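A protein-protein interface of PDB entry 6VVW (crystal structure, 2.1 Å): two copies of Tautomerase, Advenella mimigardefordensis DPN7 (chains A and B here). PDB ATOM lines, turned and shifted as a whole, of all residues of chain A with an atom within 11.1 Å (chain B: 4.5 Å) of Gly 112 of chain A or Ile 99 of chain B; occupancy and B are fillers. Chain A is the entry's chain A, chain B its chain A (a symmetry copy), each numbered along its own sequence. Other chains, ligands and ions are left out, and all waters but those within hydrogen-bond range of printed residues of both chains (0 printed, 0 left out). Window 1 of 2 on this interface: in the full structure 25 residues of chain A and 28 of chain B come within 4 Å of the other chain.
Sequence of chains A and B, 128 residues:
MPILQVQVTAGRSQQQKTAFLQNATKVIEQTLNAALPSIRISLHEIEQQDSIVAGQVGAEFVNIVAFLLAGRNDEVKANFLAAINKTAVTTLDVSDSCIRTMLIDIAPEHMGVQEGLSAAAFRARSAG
Of the 14 printed residues of chain B, 9 touch a printed residue of chain A.
Hydrophobic or aromatic side chains of chain B within 4 Å of the printed part of chain A: Leu 81.
Printed residues of chain A that touch a printed residue of chain B: Ile 3, Pro 37, Arg 40, Glu 109, Met 111, Gly 112, Val 113, Gln 114, Glu 115 and Gly 116.
Among the printed residues, 20 pairs touch across the chains.
The backbone NH of Gln 114 of chain A sits close to the guanidinium group of Arg 100 of chain B (3.5 Å).
O of Cys 98 of chain B lies within hydrogen-bond range of NH1 of Arg 40 of chain A, 2.7 Å away.
O of Val 62 of chain B lies close to NH1 of Arg 40 of chain A (2.3 Å).
The backbone carbonyl oxygen (O) of Gly 112 of chain A lies within hydrogen-bond range of the backbone NH (N) of Thr 101 of chain B, 2.7 Å away.
O of Ile 99 of chain B sits close to O of Gly 112 of chain A (3.2 Å).
The backbone carbonyl oxygen of Met 111 of chain A sits at hydrogen-bond distance from the backbone NH of Ala 119 of chain A (2.8 Å).
N of Val 62 of chain B sits at hydrogen-bond distance from O of Cys 98 of chain B (3.2 Å).
N of Ile 64 of chain B sits at hydrogen-bond distance from O of Arg 100 of chain B, at 2.8 Å.
The side-chain hydroxyl (OG) of Ser 95 of chain B lies close to the backbone NH (N) of Ser 97 of chain B.
The side-chain hydroxyl of Ser 95 of chain B is in hydrogen-bond range of the side-chain carboxylate of Asp 96 of chain B (2.7 Å).
Of the printed residues of chain B, Gly 112 of chain A touches Leu 81 (3.7 Å), Ile 99 (3.2 Å), Arg 100 (3.4 Å) and Thr 101 (2.7 Å).
Val 62 of chain B touches one residue of chain A.
No residue of chain A comes within 4 Å of Ile 64 of chain B.
No residue of chain A comes within 4 Å of Ala 88 of chain B.
Ser 97 of chain B touches just one residue of chain A: Gln 114.
Of chain A, only Met 111 and Gly 112 come within 4 Å of Thr 101 of chain B.
Of the printed residues of chain B, Val 113 of chain A touches Asn 85, Ile 99 and Arg 100.
Printed residues of chain B within 4 Å of Pro 37 of chain A: Arg 100.
Printed residues of chain A within 4 Å of Asp 96 of chain B: Glu 115 (3.7 Å).
Printed residues of chain A within 4 Å of Leu 81 of chain B: Glu 109, Gly 112 and Gly 116.
Ala 120 of chain A touches none of the printed residues of chain B.
The nearest printed residue of chain B that does not touch Gly 112 of chain A is Asn 85 of chain B (6.1 Å).
The nearest residue of chain A that does not touch Ile 99 of chain B is Arg 40 of chain A (4.1 Å).
The nearest printed residue of chain B that does not touch Gly 116 of chain A is Asp 96 of chain B (4.8 Å).
No position is printed for both chains.
Of the 20 pairs that touch across the chains among the printed residues, none has its exchanged pair printed and touching as well.
Among the printed residues, pairs that only touch across the chains: Ile 3 of chain A with Arg 100 of chain B, Pro 37 of chain A with Arg 100 of chain B, Arg 40 of chain A with Arg 100 of chain B, Glu 109 of chain A with Leu 81 of chain B, Met 111 of chain A with Thr 101 of chain B, Gly 112 of chain A with Leu 81 of chain B, Gly 112 of chain A with Arg 100 of chain B, Val 113 of chain A with Asn 85 of chain B, Val 113 of chain A with Ile 99 of chain B, Val 113 of chain A with Arg 100 of chain B, Gln 114 of chain A with Ser 97 of chain B, Glu 115 of chain A with Asn 85 of chain B, Glu 115 of chain A with Asp 96 of chain B, Gly 116 of chain A with Leu 81 of chain B and Gly 116 of chain A with Asn 85 of chain B.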
ATOM      1  N   ILE A   3      18.274  19.902 -35.193  1.00  0.00           N
ATOM      2  CA  ILE A   3      17.887  18.953 -36.219  1.00  0.00           C
ATOM      3  C   ILE A   3      17.171  19.700 -37.334  1.00  0.00           C
ATOM      4  O   ILE A   3      16.476  20.691 -37.109  1.00  0.00           O
ATOM      5  CB  ILE A   3      17.017  17.843 -35.619  1.00  0.00           C
ATOM      6  CG1 ILE A   3      15.564  18.247 -35.621  1.00  0.00           C
ATOM      7  CG2 ILE A   3      17.448  17.593 -34.204  1.00  0.00           C
ATOM      8  CD1 ILE A   3      14.709  17.184 -35.134  1.00  0.00           C
ATOM      9  N   GLN A   5      14.978  19.398 -41.109  1.00  0.00           N
ATOM     10  CA  GLN A   5      14.258  18.647 -42.121  1.00  0.00           C
ATOM     11  C   GLN A   5      14.086  19.594 -43.282  1.00  0.00           C
ATOM     12  O   GLN A   5      13.889  20.794 -43.073  1.00  0.00           O
ATOM     13  CB  GLN A   5      12.889  18.134 -41.617  1.00  0.00           C
ATOM     14  CG  GLN A   5      12.969  17.380 -40.316  1.00  0.00           C
ATOM     15  CD  GLN A   5      11.664  16.720 -39.931  1.00  0.00           C
ATOM     16  OE1 GLN A   5      10.626  16.954 -40.555  1.00  0.00           O
ATOM     17  NE2 GLN A   5      11.712  15.862 -38.913  1.00  0.00           N
ATOM     18  N   PRO A  37      27.369  16.343 -32.468  1.00  0.00           N
ATOM     19  CA  PRO A  37      26.368  15.303 -32.171  1.00  0.00           C
ATOM     20  C   PRO A  37      24.947  15.798 -32.005  1.00  0.00           C
ATOM     21  O   PRO A  37      24.005  15.000 -31.983  1.00  0.00           O
ATOM     22  CB  PRO A  37      26.869  14.704 -30.855  1.00  0.00           C
ATOM     23  CG  PRO A  37      28.306  15.024 -30.808  1.00  0.00           C
ATOM     24  CD  PRO A  37      28.464  16.334 -31.483  1.00  0.00           C
ATOM     25  N   SER A  38      24.792  17.114 -31.879  1.00  0.00           N
ATOM     26  CA  SER A  38      23.487  17.729 -31.681  1.00  0.00           C
ATOM     27  C   SER A  38      22.745  17.937 -32.988  1.00  0.00           C
ATOM     28  O   SER A  38      21.510  17.913 -33.017  1.00  0.00           O
ATOM     29  CB  SER A  38      23.674  19.070 -30.984  1.00  0.00           C
ATOM     30  OG  SER A  38      24.819  19.723 -31.516  1.00  0.00           O
ATOM     31  N   ILE A  39      23.450  18.143 -34.037  1.00  0.00           N
ATOM     32  CA  ILE A  39      22.839  18.473 -35.307  1.00  0.00           C
ATOM     33  C   ILE A  39      22.485  17.197 -36.030  1.00  0.00           C
ATOM     34  O   ILE A  39      23.200  16.197 -35.944  1.00  0.00           O
ATOM     35  CB  ILE A  39      23.790  19.326 -36.154  1.00  0.00           C
ATOM     36  CG1 ILE A  39      24.418  20.420 -35.281  1.00  0.00           C
ATOM     37  CG2 ILE A  39      23.048  19.867 -37.359  1.00  0.00           C
ATOM     38  CD1 ILE A  39      25.820  20.827 -35.691  1.00  0.00           C
ATOM     39  N   ARG A  40      21.361  17.225 -36.729  1.00  0.00           N
ATOM     40  CA  ARG A  40      21.072  16.269 -37.775  1.00  0.00           C
ATOM     41  C   ARG A  40      20.398  17.030 -38.897  1.00  0.00           C
ATOM     42  O   ARG A  40      19.943  18.159 -38.718  1.00  0.00           O
ATOM     43  CB  ARG A  40      20.196  15.101 -37.282  1.00  0.00           C
ATOM     44  CG  ARG A  40      19.320  15.425 -36.097  1.00  0.00           C
ATOM     45  CD  ARG A  40      18.420  14.266 -35.700  1.00  0.00           C
ATOM     46  NE  ARG A  40      19.118  13.320 -34.837  1.00  0.00           N
ATOM     47  CZ  ARG A  40      18.609  12.177 -34.379  1.00  0.00           C
ATOM     48  NH1 ARG A  40      17.381  11.781 -34.695  1.00  0.00           N
ATOM     49  NH2 ARG A  40      19.352  11.403 -33.610  1.00  0.00           N
ATOM     50  N   PHE A  67      14.946  22.925 -36.200  1.00  0.00           N
ATOM     51  CA  PHE A  67      14.652  22.846 -34.788  1.00  0.00           C
ATOM     52  C   PHE A  67      15.947  23.034 -34.013  1.00  0.00           C
ATOM     53  O   PHE A  67      16.877  22.230 -34.145  1.00  0.00           O
ATOM     54  CB  PHE A  67      13.997  21.509 -34.465  1.00  0.00           C
ATOM     55  CG  PHE A  67      12.673  21.321 -35.139  1.00  0.00           C
ATOM     56  CD1 PHE A  67      11.506  21.728 -34.528  1.00  0.00           C
ATOM     57  CD2 PHE A  67      12.594  20.741 -36.389  1.00  0.00           C
ATOM     58  CE1 PHE A  67      10.280  21.559 -35.153  1.00  0.00           C
ATOM     59  CE2 PHE A  67      11.378  20.574 -37.014  1.00  0.00           C
ATOM     60  CZ  PHE A  67      10.217  20.981 -36.396  1.00  0.00           C
ATOM     61  N   LEU A  68      16.016  24.117 -33.230  1.00  0.00           N
ATOM     62  CA  LEU A  68      17.200  24.439 -32.445  1.00  0.00           C
ATOM     63  C   LEU A  68      16.778  24.624 -30.998  1.00  0.00           C
ATOM     64  O   LEU A  68      15.604  24.782 -30.717  1.00  0.00           O
ATOM     65  CB  LEU A  68      17.874  25.689 -32.969  1.00  0.00           C
ATOM     66  CG  LEU A  68      17.967  25.816 -34.484  1.00  0.00           C
ATOM     67  CD1 LEU A  68      16.724  26.477 -35.090  1.00  0.00           C
ATOM     68  CD2 LEU A  68      19.191  26.614 -34.811  1.00  0.00           C
ATOM     69  N   LEU A  69      17.725  24.589 -30.073  1.00  0.00           N
ATOM     70  CA  LEU A  69      17.413  24.816 -28.661  1.00  0.00           C
ATOM     71  C   LEU A  69      17.381  26.312 -28.364  1.00  0.00           C
ATOM     72  O   LEU A  69      18.392  27.001 -28.533  1.00  0.00           O
ATOM     73  CB  LEU A  69      18.441  24.135 -27.762  1.00  0.00           C
ATOM     74  CG  LEU A  69      18.196  22.662 -27.457  1.00  0.00           C
ATOM     75  CD1 LEU A  69      19.527  21.971 -27.222  1.00  0.00           C
ATOM     76  CD2 LEU A  69      17.269  22.486 -26.272  1.00  0.00           C
ATOM     77  N   ILE A 106      13.241  25.665 -29.538  1.00  0.00           N
ATOM     78  CA  ILE A 106      12.617  24.746 -28.596  1.00  0.00           C
ATOM     79  C   ILE A 106      13.243  24.931 -27.220  1.00  0.00           C
ATOM     80  O   ILE A 106      14.432  25.253 -27.068  1.00  0.00           O
ATOM     81  CB  ILE A 106      12.741  23.275 -29.063  1.00  0.00           C
ATOM     82  CG1 ILE A 106      11.433  22.530 -28.856  1.00  0.00           C
ATOM     83  CG2 ILE A 106      13.844  22.529 -28.293  1.00  0.00           C
ATOM     84  CD1 ILE A 106      11.624  21.029 -28.676  1.00  0.00           C
ATOM     85  N   ALA A 107      12.489  24.742 -26.288  1.00  0.00           N
ATOM     86  CA  ALA A 107      12.842  24.908 -24.897  1.00  0.00           C
ATOM     87  C   ALA A 107      13.452  23.621 -24.374  1.00  0.00           C
ATOM     88  O   ALA A 107      13.096  22.537 -24.829  1.00  0.00           O
ATOM     89  CB  ALA A 107      11.600  25.264 -24.077  1.00  0.00           C
ATOM     90  N   PRO A 108      14.367  23.723 -23.418  1.00  0.00           N
ATOM     91  CA  PRO A 108      15.149  22.551 -23.040  1.00  0.00           C
ATOM     92  C   PRO A 108      14.335  21.445 -22.414  1.00  0.00           C
ATOM     93  O   PRO A 108      14.778  20.289 -22.436  1.00  0.00           O
ATOM     94  CB  PRO A 108      16.173  23.133 -22.067  1.00  0.00           C
ATOM     95  CG  PRO A 108      16.348  24.547 -22.545  1.00  0.00           C
ATOM     96  CD  PRO A 108      14.968  24.971 -22.915  1.00  0.00           C
ATOM     97  N   GLU A 109      13.165  21.754 -21.858  1.00  0.00           N
ATOM     98  CA  GLU A 109      12.263  20.757 -21.294  1.00  0.00           C
ATOM     99  C   GLU A 109      11.329  20.163 -22.323  1.00  0.00           C
ATOM    100  O   GLU A 109      10.583  19.233 -21.994  1.00  0.00           O
ATOM    101  CB  GLU A 109      11.390  21.355 -20.186  1.00  0.00           C
ATOM    102  CG  GLU A 109      12.139  22.161 -19.179  1.00  0.00           C
ATOM    103  CD  GLU A 109      12.171  23.595 -19.551  1.00  0.00           C
ATOM    104  OE1 GLU A 109      11.232  24.028 -20.241  1.00  0.00           O
ATOM    105  OE2 GLU A 109      13.132  24.290 -19.161  1.00  0.00           O
ATOM    106  N   HIS A 110      11.308  20.703 -23.534  1.00  0.00           N
ATOM    107  CA  HIS A 110      10.379  20.240 -24.546  1.00  0.00           C
ATOM    108  C   HIS A 110      11.065  19.498 -25.684  1.00  0.00           C
ATOM    109  O   HIS A 110      10.397  19.112 -26.641  1.00  0.00           O
ATOM    110  CB  HIS A 110       9.578  21.420 -25.076  1.00  0.00           C
ATOM    111  CG  HIS A 110       8.622  21.970 -24.072  1.00  0.00           C
ATOM    112  ND1 HIS A 110       8.189  23.278 -24.085  1.00  0.00           N
ATOM    113  CD2 HIS A 110       8.029  21.389 -23.005  1.00  0.00           C
ATOM    114  CE1 HIS A 110       7.355  23.474 -23.079  1.00  0.00           C
ATOM    115  NE2 HIS A 110       7.247  22.344 -22.405  1.00  0.00           N
ATOM    116  N   MET A 111      12.366  19.278 -25.605  1.00  0.00           N
ATOM    117  CA  MET A 111      13.067  18.458 -26.579  1.00  0.00           C
ATOM    118  C   MET A 111      13.480  17.173 -25.897  1.00  0.00           C
ATOM    119  O   MET A 111      14.188  17.204 -24.887  1.00  0.00           O
ATOM    120  CB  MET A 111      14.290  19.167 -27.146  1.00  0.00           C
ATOM    121  CG  MET A 111      14.543  18.777 -28.580  1.00  0.00           C
ATOM    122  SD  MET A 111      15.905  19.678 -29.296  1.00  0.00           S
ATOM    123  CE  MET A 111      15.273  20.157 -30.893  1.00  0.00           C
ATOM    124  N   GLY A 112      13.029  16.050 -26.433  1.00  0.00           N
ATOM    125  CA  GLY A 112      13.393  14.760 -25.874  1.00  0.00           C
ATOM    126  C   GLY A 112      14.587  14.210 -26.610  1.00  0.00           C
ATOM    127  O   GLY A 112      14.534  13.998 -27.822  1.00  0.00           O
ATOM    128  N   VAL A 113      15.684  14.001 -25.899  1.00  0.00           N
ATOM    129  CA  VAL A 113      16.938  13.696 -26.563  1.00  0.00           C
ATOM    130  C   VAL A 113      17.454  12.356 -26.048  1.00  0.00           C
ATOM    131  O   VAL A 113      16.657  11.460 -25.746  1.00  0.00           O
ATOM    132  CB  VAL A 113      17.919  14.863 -26.362  1.00  0.00           C
ATOM    133  CG1 VAL A 113      17.269  16.151 -26.856  1.00  0.00           C
ATOM    134  CG2 VAL A 113      18.288  15.020 -24.909  1.00  0.00           C
ATOM    135  N   GLN A 114      18.773  12.193 -25.974  1.00  0.00           N
ATOM    136  CA  GLN A 114      19.368  10.975 -25.444  1.00  0.00           C
ATOM    137  C   GLN A 114      18.603  10.453 -24.234  1.00  0.00           C
ATOM    138  O   GLN A 114      18.206  11.219 -23.356  1.00  0.00           O
ATOM    139  CB  GLN A 114      20.818  11.241 -25.055  1.00  0.00           C
ATOM    140  CG  GLN A 114      21.711  11.701 -26.189  1.00  0.00           C
ATOM    141  CD  GLN A 114      22.144  13.148 -26.052  1.00  0.00           C
ATOM    142  OE1 GLN A 114      21.323  14.031 -25.791  1.00  0.00           O
ATOM    143  NE2 GLN A 114      23.442  13.397 -26.231  1.00  0.00           N
ATOM    144  N   GLU A 115      18.348   9.146 -24.227  1.00  0.00           N
ATOM    145  CA  GLU A 115      17.749   8.476 -23.078  1.00  0.00           C
ATOM    146  C   GLU A 115      16.314   8.912 -22.818  1.00  0.00           C
ATOM    147  O   GLU A 115      15.684   8.470 -21.855  1.00  0.00           O
ATOM    148  CB  GLU A 115      18.594   8.736 -21.841  1.00  0.00           C
ATOM    149  CG  GLU A 115      18.740   7.578 -20.909  1.00  0.00           C
ATOM    150  CD  GLU A 115      20.100   7.565 -20.272  1.00  0.00           C
ATOM    151  OE1 GLU A 115      20.524   6.493 -19.800  1.00  0.00           O
ATOM    152  OE2 GLU A 115      20.759   8.629 -20.270  1.00  0.00           O
ATOM    153  N   GLY A 116      15.774   9.765 -23.667  1.00  0.00           N
ATOM    154  CA  GLY A 116      14.464  10.308 -23.386  1.00  0.00           C
ATOM    155  C   GLY A 116      14.406  11.255 -22.213  1.00  0.00           C
ATOM    156  O   GLY A 116      13.309  11.567 -21.746  1.00  0.00           O
ATOM    157  N   LEU A 117      15.548  11.685 -21.695  1.00  0.00           N
ATOM    158  CA  LEU A 117      15.589  12.762 -20.722  1.00  0.00           C
ATOM    159  C   LEU A 117      15.521  14.078 -21.473  1.00  0.00           C
ATOM    160  O   LEU A 117      16.232  14.259 -22.461  1.00  0.00           O
ATOM    161  CB  LEU A 117      16.874  12.685 -19.900  1.00  0.00           C
ATOM    162  CG  LEU A 117      17.170  11.362 -19.188  1.00  0.00           C
ATOM    163  CD1 LEU A 117      18.658  11.046 -19.213  1.00  0.00           C
ATOM    164  CD2 LEU A 117      16.666  11.385 -17.747  1.00  0.00           C
ATOM    165  N   SER A 118      14.651  14.984 -21.032  1.00  0.00           N
ATOM    166  CA  SER A 118      14.513  16.253 -21.726  1.00  0.00           C
ATOM    167  C   SER A 118      15.867  16.950 -21.809  1.00  0.00           C
ATOM    168  O   SER A 118      16.795  16.655 -21.052  1.00  0.00           O
ATOM    169  CB  SER A 118      13.479  17.141 -21.032  1.00  0.00           C
ATOM    170  OG  SER A 118      13.979  17.693 -19.826  1.00  0.00           O
ATOM    171  N   ALA A 119      15.994  17.849 -22.786  1.00  0.00           N
ATOM    172  CA  ALA A 119      17.258  18.549 -22.964  1.00  0.00           C
ATOM    173  C   ALA A 119      17.583  19.421 -21.759  1.00  0.00           C
ATOM    174  O   ALA A 119      18.759  19.674 -21.474  1.00  0.00           O
ATOM    175  CB  ALA A 119      17.211  19.388 -24.232  1.00  0.00           C
ATOM    176  N   ALA A 120      16.557  19.891 -21.048  1.00  0.00           N
ATOM    177  CA  ALA A 120      16.772  20.696 -19.853  1.00  0.00           C
ATOM    178  C   ALA A 120      17.657  19.976 -18.856  1.00  0.00           C
ATOM    179  O   ALA A 120      18.611  20.555 -18.323  1.00  0.00           O
ATOM    180  CB  ALA A 120      15.428  21.032 -19.224  1.00  0.00           C
ATOM    181  N   ALA A 121      17.369  18.703 -18.612  1.00  0.00           N
ATOM    182  CA  ALA A 121      18.039  17.892 -17.602  1.00  0.00           C
ATOM    183  C   ALA A 121      19.522  17.671 -17.886  1.00  0.00           C
ATOM    184  O   ALA A 121      20.118  16.730 -17.350  1.00  0.00           O
ATOM    185  CB  ALA A 121      17.328  16.540 -17.474  1.00  0.00           C
ATOM    186  N   PHE A 122      20.129  18.522 -18.711  1.00  0.00           N
ATOM    187  CA  PHE A 122      21.560  18.448 -18.977  1.00  0.00           C
ATOM    188  C   PHE A 122      22.298  19.669 -18.459  1.00  0.00           C
ATOM    189  O   PHE A 122      22.788  19.655 -17.331  1.00  0.00           O
ATOM    190  CB  PHE A 122      21.807  18.278 -20.465  1.00  0.00           C
ATOM    191  CG  PHE A 122      21.692  16.860 -20.918  1.00  0.00           C
ATOM    192  CD1 PHE A 122      20.449  16.300 -21.159  1.00  0.00           C
ATOM    193  CD2 PHE A 122      22.824  16.070 -21.066  1.00  0.00           C
ATOM    194  CE1 PHE A 122      20.335  14.973 -21.559  1.00  0.00           C
ATOM    195  CE2 PHE A 122      22.717  14.734 -21.469  1.00  0.00           C
ATOM    196  CZ  PHE A 122      21.475  14.188 -21.716  1.00  0.00           C
ATOM    197  N   VAL B  62      16.008   8.768 -35.424  1.00  0.00           N
ATOM    198  CA  VAL B  62      14.588   9.063 -35.362  1.00  0.00           C
ATOM    199  C   VAL B  62      14.474  10.483 -34.868  1.00  0.00           C
ATOM    200  O   VAL B  62      15.300  10.929 -34.070  1.00  0.00           O
ATOM    201  CB  VAL B  62      13.840   8.098 -34.434  1.00  0.00           C
ATOM    202  CG1 VAL B  62      12.422   8.531 -34.265  1.00  0.00           C
ATOM    203  CG2 VAL B  62      13.882   6.675 -34.992  1.00  0.00           C
ATOM    204  N   ILE B  64      10.995  12.604 -33.628  1.00  0.00           N
ATOM    205  CA  ILE B  64       9.563  12.732 -33.470  1.00  0.00           C
ATOM    206  C   ILE B  64       9.212  14.198 -33.317  1.00  0.00           C
ATOM    207  O   ILE B  64       9.636  14.845 -32.357  1.00  0.00           O
ATOM    208  CB  ILE B  64       9.073  11.954 -32.255  1.00  0.00           C
ATOM    209  CG1 ILE B  64       9.630  10.554 -32.284  1.00  0.00           C
ATOM    210  CG2 ILE B  64       7.574  11.946 -32.257  1.00  0.00           C
ATOM    211  CD1 ILE B  64       8.944   9.657 -31.326  1.00  0.00           C
ATOM    212  N   LEU B  81       8.287  11.973 -23.364  1.00  0.00           N
ATOM    213  CA  LEU B  81       9.623  11.824 -23.926  1.00  0.00           C
ATOM    214  C   LEU B  81      10.278  10.518 -23.494  1.00  0.00           C
ATOM    215  O   LEU B  81      10.909   9.830 -24.307  1.00  0.00           O
ATOM    216  CB  LEU B  81      10.477  13.027 -23.523  1.00  0.00           C
ATOM    217  CG  LEU B  81       9.772  14.334 -23.866  1.00  0.00           C
ATOM    218  CD1 LEU B  81      10.615  15.563 -23.553  1.00  0.00           C
ATOM    219  CD2 LEU B  81       9.402  14.289 -25.319  1.00  0.00           C
ATOM    220  N   ASN B  85      10.693   7.534 -26.215  1.00  0.00           N
ATOM    221  CA  ASN B  85      12.025   7.006 -26.475  1.00  0.00           C
ATOM    222  C   ASN B  85      12.098   5.527 -26.103  1.00  0.00           C
ATOM    223  O   ASN B  85      12.735   4.738 -26.806  1.00  0.00           O
ATOM    224  CB  ASN B  85      13.061   7.838 -25.718  1.00  0.00           C
ATOM    225  CG  ASN B  85      14.473   7.340 -25.899  1.00  0.00           C
ATOM    226  OD1 ASN B  85      14.885   6.380 -25.257  1.00  0.00           O
ATOM    227  ND2 ASN B  85      15.237   8.017 -26.743  1.00  0.00           N
ATOM    228  N   ALA B  88      10.187   3.699 -29.040  1.00  0.00           N
ATOM    229  CA  ALA B  88      10.990   3.807 -30.245  1.00  0.00           C
ATOM    230  C   ALA B  88      12.175   2.871 -30.183  1.00  0.00           C
ATOM    231  O   ALA B  88      12.498   2.190 -31.162  1.00  0.00           O
ATOM    232  CB  ALA B  88      11.462   5.242 -30.428  1.00  0.00           C
ATOM    233  N   VAL B  89      12.840   2.822 -29.037  1.00  0.00           N
ATOM    234  CA  VAL B  89      13.955   1.904 -28.887  1.00  0.00           C
ATOM    235  C   VAL B  89      13.477   0.461 -29.008  1.00  0.00           C
ATOM    236  O   VAL B  89      13.974  -0.305 -29.844  1.00  0.00           O
ATOM    237  CB  VAL B  89      14.671   2.152 -27.554  1.00  0.00           C
ATOM    238  CG1 VAL B  89      15.534   0.971 -27.217  1.00  0.00           C
ATOM    239  CG2 VAL B  89      15.512   3.382 -27.653  1.00  0.00           C
ATOM    240  N   VAL B  94      16.735   0.643 -32.325  1.00  0.00           N
ATOM    241  CA  VAL B  94      17.661   1.744 -32.505  1.00  0.00           C
ATOM    242  C   VAL B  94      18.226   2.101 -31.133  1.00  0.00           C
ATOM    243  O   VAL B  94      17.960   1.417 -30.140  1.00  0.00           O
ATOM    244  CB  VAL B  94      16.978   2.943 -33.199  1.00  0.00           C
ATOM    245  CG1 VAL B  94      16.253   3.841 -32.197  1.00  0.00           C
ATOM    246  CG2 VAL B  94      17.964   3.705 -34.050  1.00  0.00           C
ATOM    247  N   SER B  95      19.052   3.146 -31.071  1.00  0.00           N
ATOM    248  CA  SER B  95      19.606   3.561 -29.790  1.00  0.00           C
ATOM    249  C   SER B  95      18.710   4.603 -29.148  1.00  0.00           C
ATOM    250  O   SER B  95      17.996   5.337 -29.831  1.00  0.00           O
ATOM    251  CB  SER B  95      21.016   4.131 -29.935  1.00  0.00           C
ATOM    252  OG  SER B  95      21.547   4.457 -28.653  1.00  0.00           O
ATOM    253  N   ASP B  96      18.738   4.633 -27.813  1.00  0.00           N
ATOM    254  CA  ASP B  96      18.041   5.678 -27.070  1.00  0.00           C
ATOM    255  C   ASP B  96      18.534   7.054 -27.476  1.00  0.00           C
ATOM    256  O   ASP B  96      17.735   7.975 -27.698  1.00  0.00           O
ATOM    257  CB  ASP B  96      18.266   5.462 -25.578  1.00  0.00           C
ATOM    258  CG  ASP B  96      19.717   5.233 -25.258  1.00  0.00           C
ATOM    259  OD1 ASP B  96      20.449   4.775 -26.174  1.00  0.00           O
ATOM    260  OD2 ASP B  96      20.129   5.512 -24.111  1.00  0.00           O
ATOM    261  N   SER B  97      19.856   7.196 -27.601  1.00  0.00           N
ATOM    262  CA  SER B  97      20.503   8.481 -27.820  1.00  0.00           C
ATOM    263  C   SER B  97      20.115   9.155 -29.121  1.00  0.00           C
ATOM    264  O   SER B  97      20.318  10.368 -29.250  1.00  0.00           O
ATOM    265  CB  SER B  97      22.010   8.304 -27.827  1.00  0.00           C
ATOM    266  OG  SER B  97      22.572   9.256 -28.717  1.00  0.00           O
ATOM    267  N   CYS B  98      19.593   8.412 -30.100  1.00  0.00           N
ATOM    268  CA  CYS B  98      19.468   8.925 -31.460  1.00  0.00           C
ATOM    269  C   CYS B  98      18.071   9.399 -31.792  1.00  0.00           C
ATOM    270  O   CYS B  98      17.821   9.798 -32.938  1.00  0.00           O
ATOM    271  CB  CYS B  98      19.875   7.863 -32.482  1.00  0.00           C
ATOM    272  SG  CYS B  98      18.512   6.842 -33.013  1.00  0.00           S
ATOM    273  N   ILE B  99      17.165   9.376 -30.828  1.00  0.00           N
ATOM    274  CA  ILE B  99      15.806   9.853 -31.031  1.00  0.00           C
ATOM    275  C   ILE B  99      15.719  11.302 -30.583  1.00  0.00           C
ATOM    276  O   ILE B  99      16.027  11.626 -29.434  1.00  0.00           O
ATOM    277  CB  ILE B  99      14.806   8.981 -30.272  1.00  0.00           C
ATOM    278  CG1 ILE B  99      14.688   7.621 -30.989  1.00  0.00           C
ATOM    279  CG2 ILE B  99      13.471   9.715 -30.147  1.00  0.00           C
ATOM    280  CD1 ILE B  99      14.906   6.414 -30.098  1.00  0.00           C
ATOM    281  N   ARG B 100      15.321  12.179 -31.484  1.00  0.00           N
ATOM    282  CA  ARG B 100      15.135  13.572 -31.144  1.00  0.00           C
ATOM    283  C   ARG B 100      13.651  13.853 -31.203  1.00  0.00           C
ATOM    284  O   ARG B 100      13.069  13.892 -32.284  1.00  0.00           O
ATOM    285  CB  ARG B 100      15.905  14.474 -32.091  1.00  0.00           C
ATOM    286  CG  ARG B 100      17.341  14.370 -31.861  1.00  0.00           C
ATOM    287  CD  ARG B 100      17.622  14.409 -30.380  1.00  0.00           C
ATOM    288  NE  ARG B 100      19.014  14.744 -30.151  1.00  0.00           N
ATOM    289  CZ  ARG B 100      19.918  13.903 -29.665  1.00  0.00           C
ATOM    290  NH1 ARG B 100      19.574  12.676 -29.334  1.00  0.00           N
ATOM    291  NH2 ARG B 100      21.170  14.295 -29.513  1.00  0.00           N
ATOM    292  N   THR B 101      13.039  14.036 -30.051  1.00  0.00           N
ATOM    293  CA  THR B 101      11.643  14.420 -29.997  1.00  0.00           C
ATOM    294  C   THR B 101      11.534  15.924 -29.820  1.00  0.00           C
ATOM    295  O   THR B 101      12.474  16.598 -29.400  1.00  0.00           O
ATOM    296  CB  THR B 101      10.937  13.692 -28.868  1.00  0.00           C
ATOM    297  OG1 THR B 101      11.406  12.346 -28.856  1.00  0.00           O
ATOM    298  CG2 THR B 101       9.450  13.677 -29.084  1.00  0.00           C
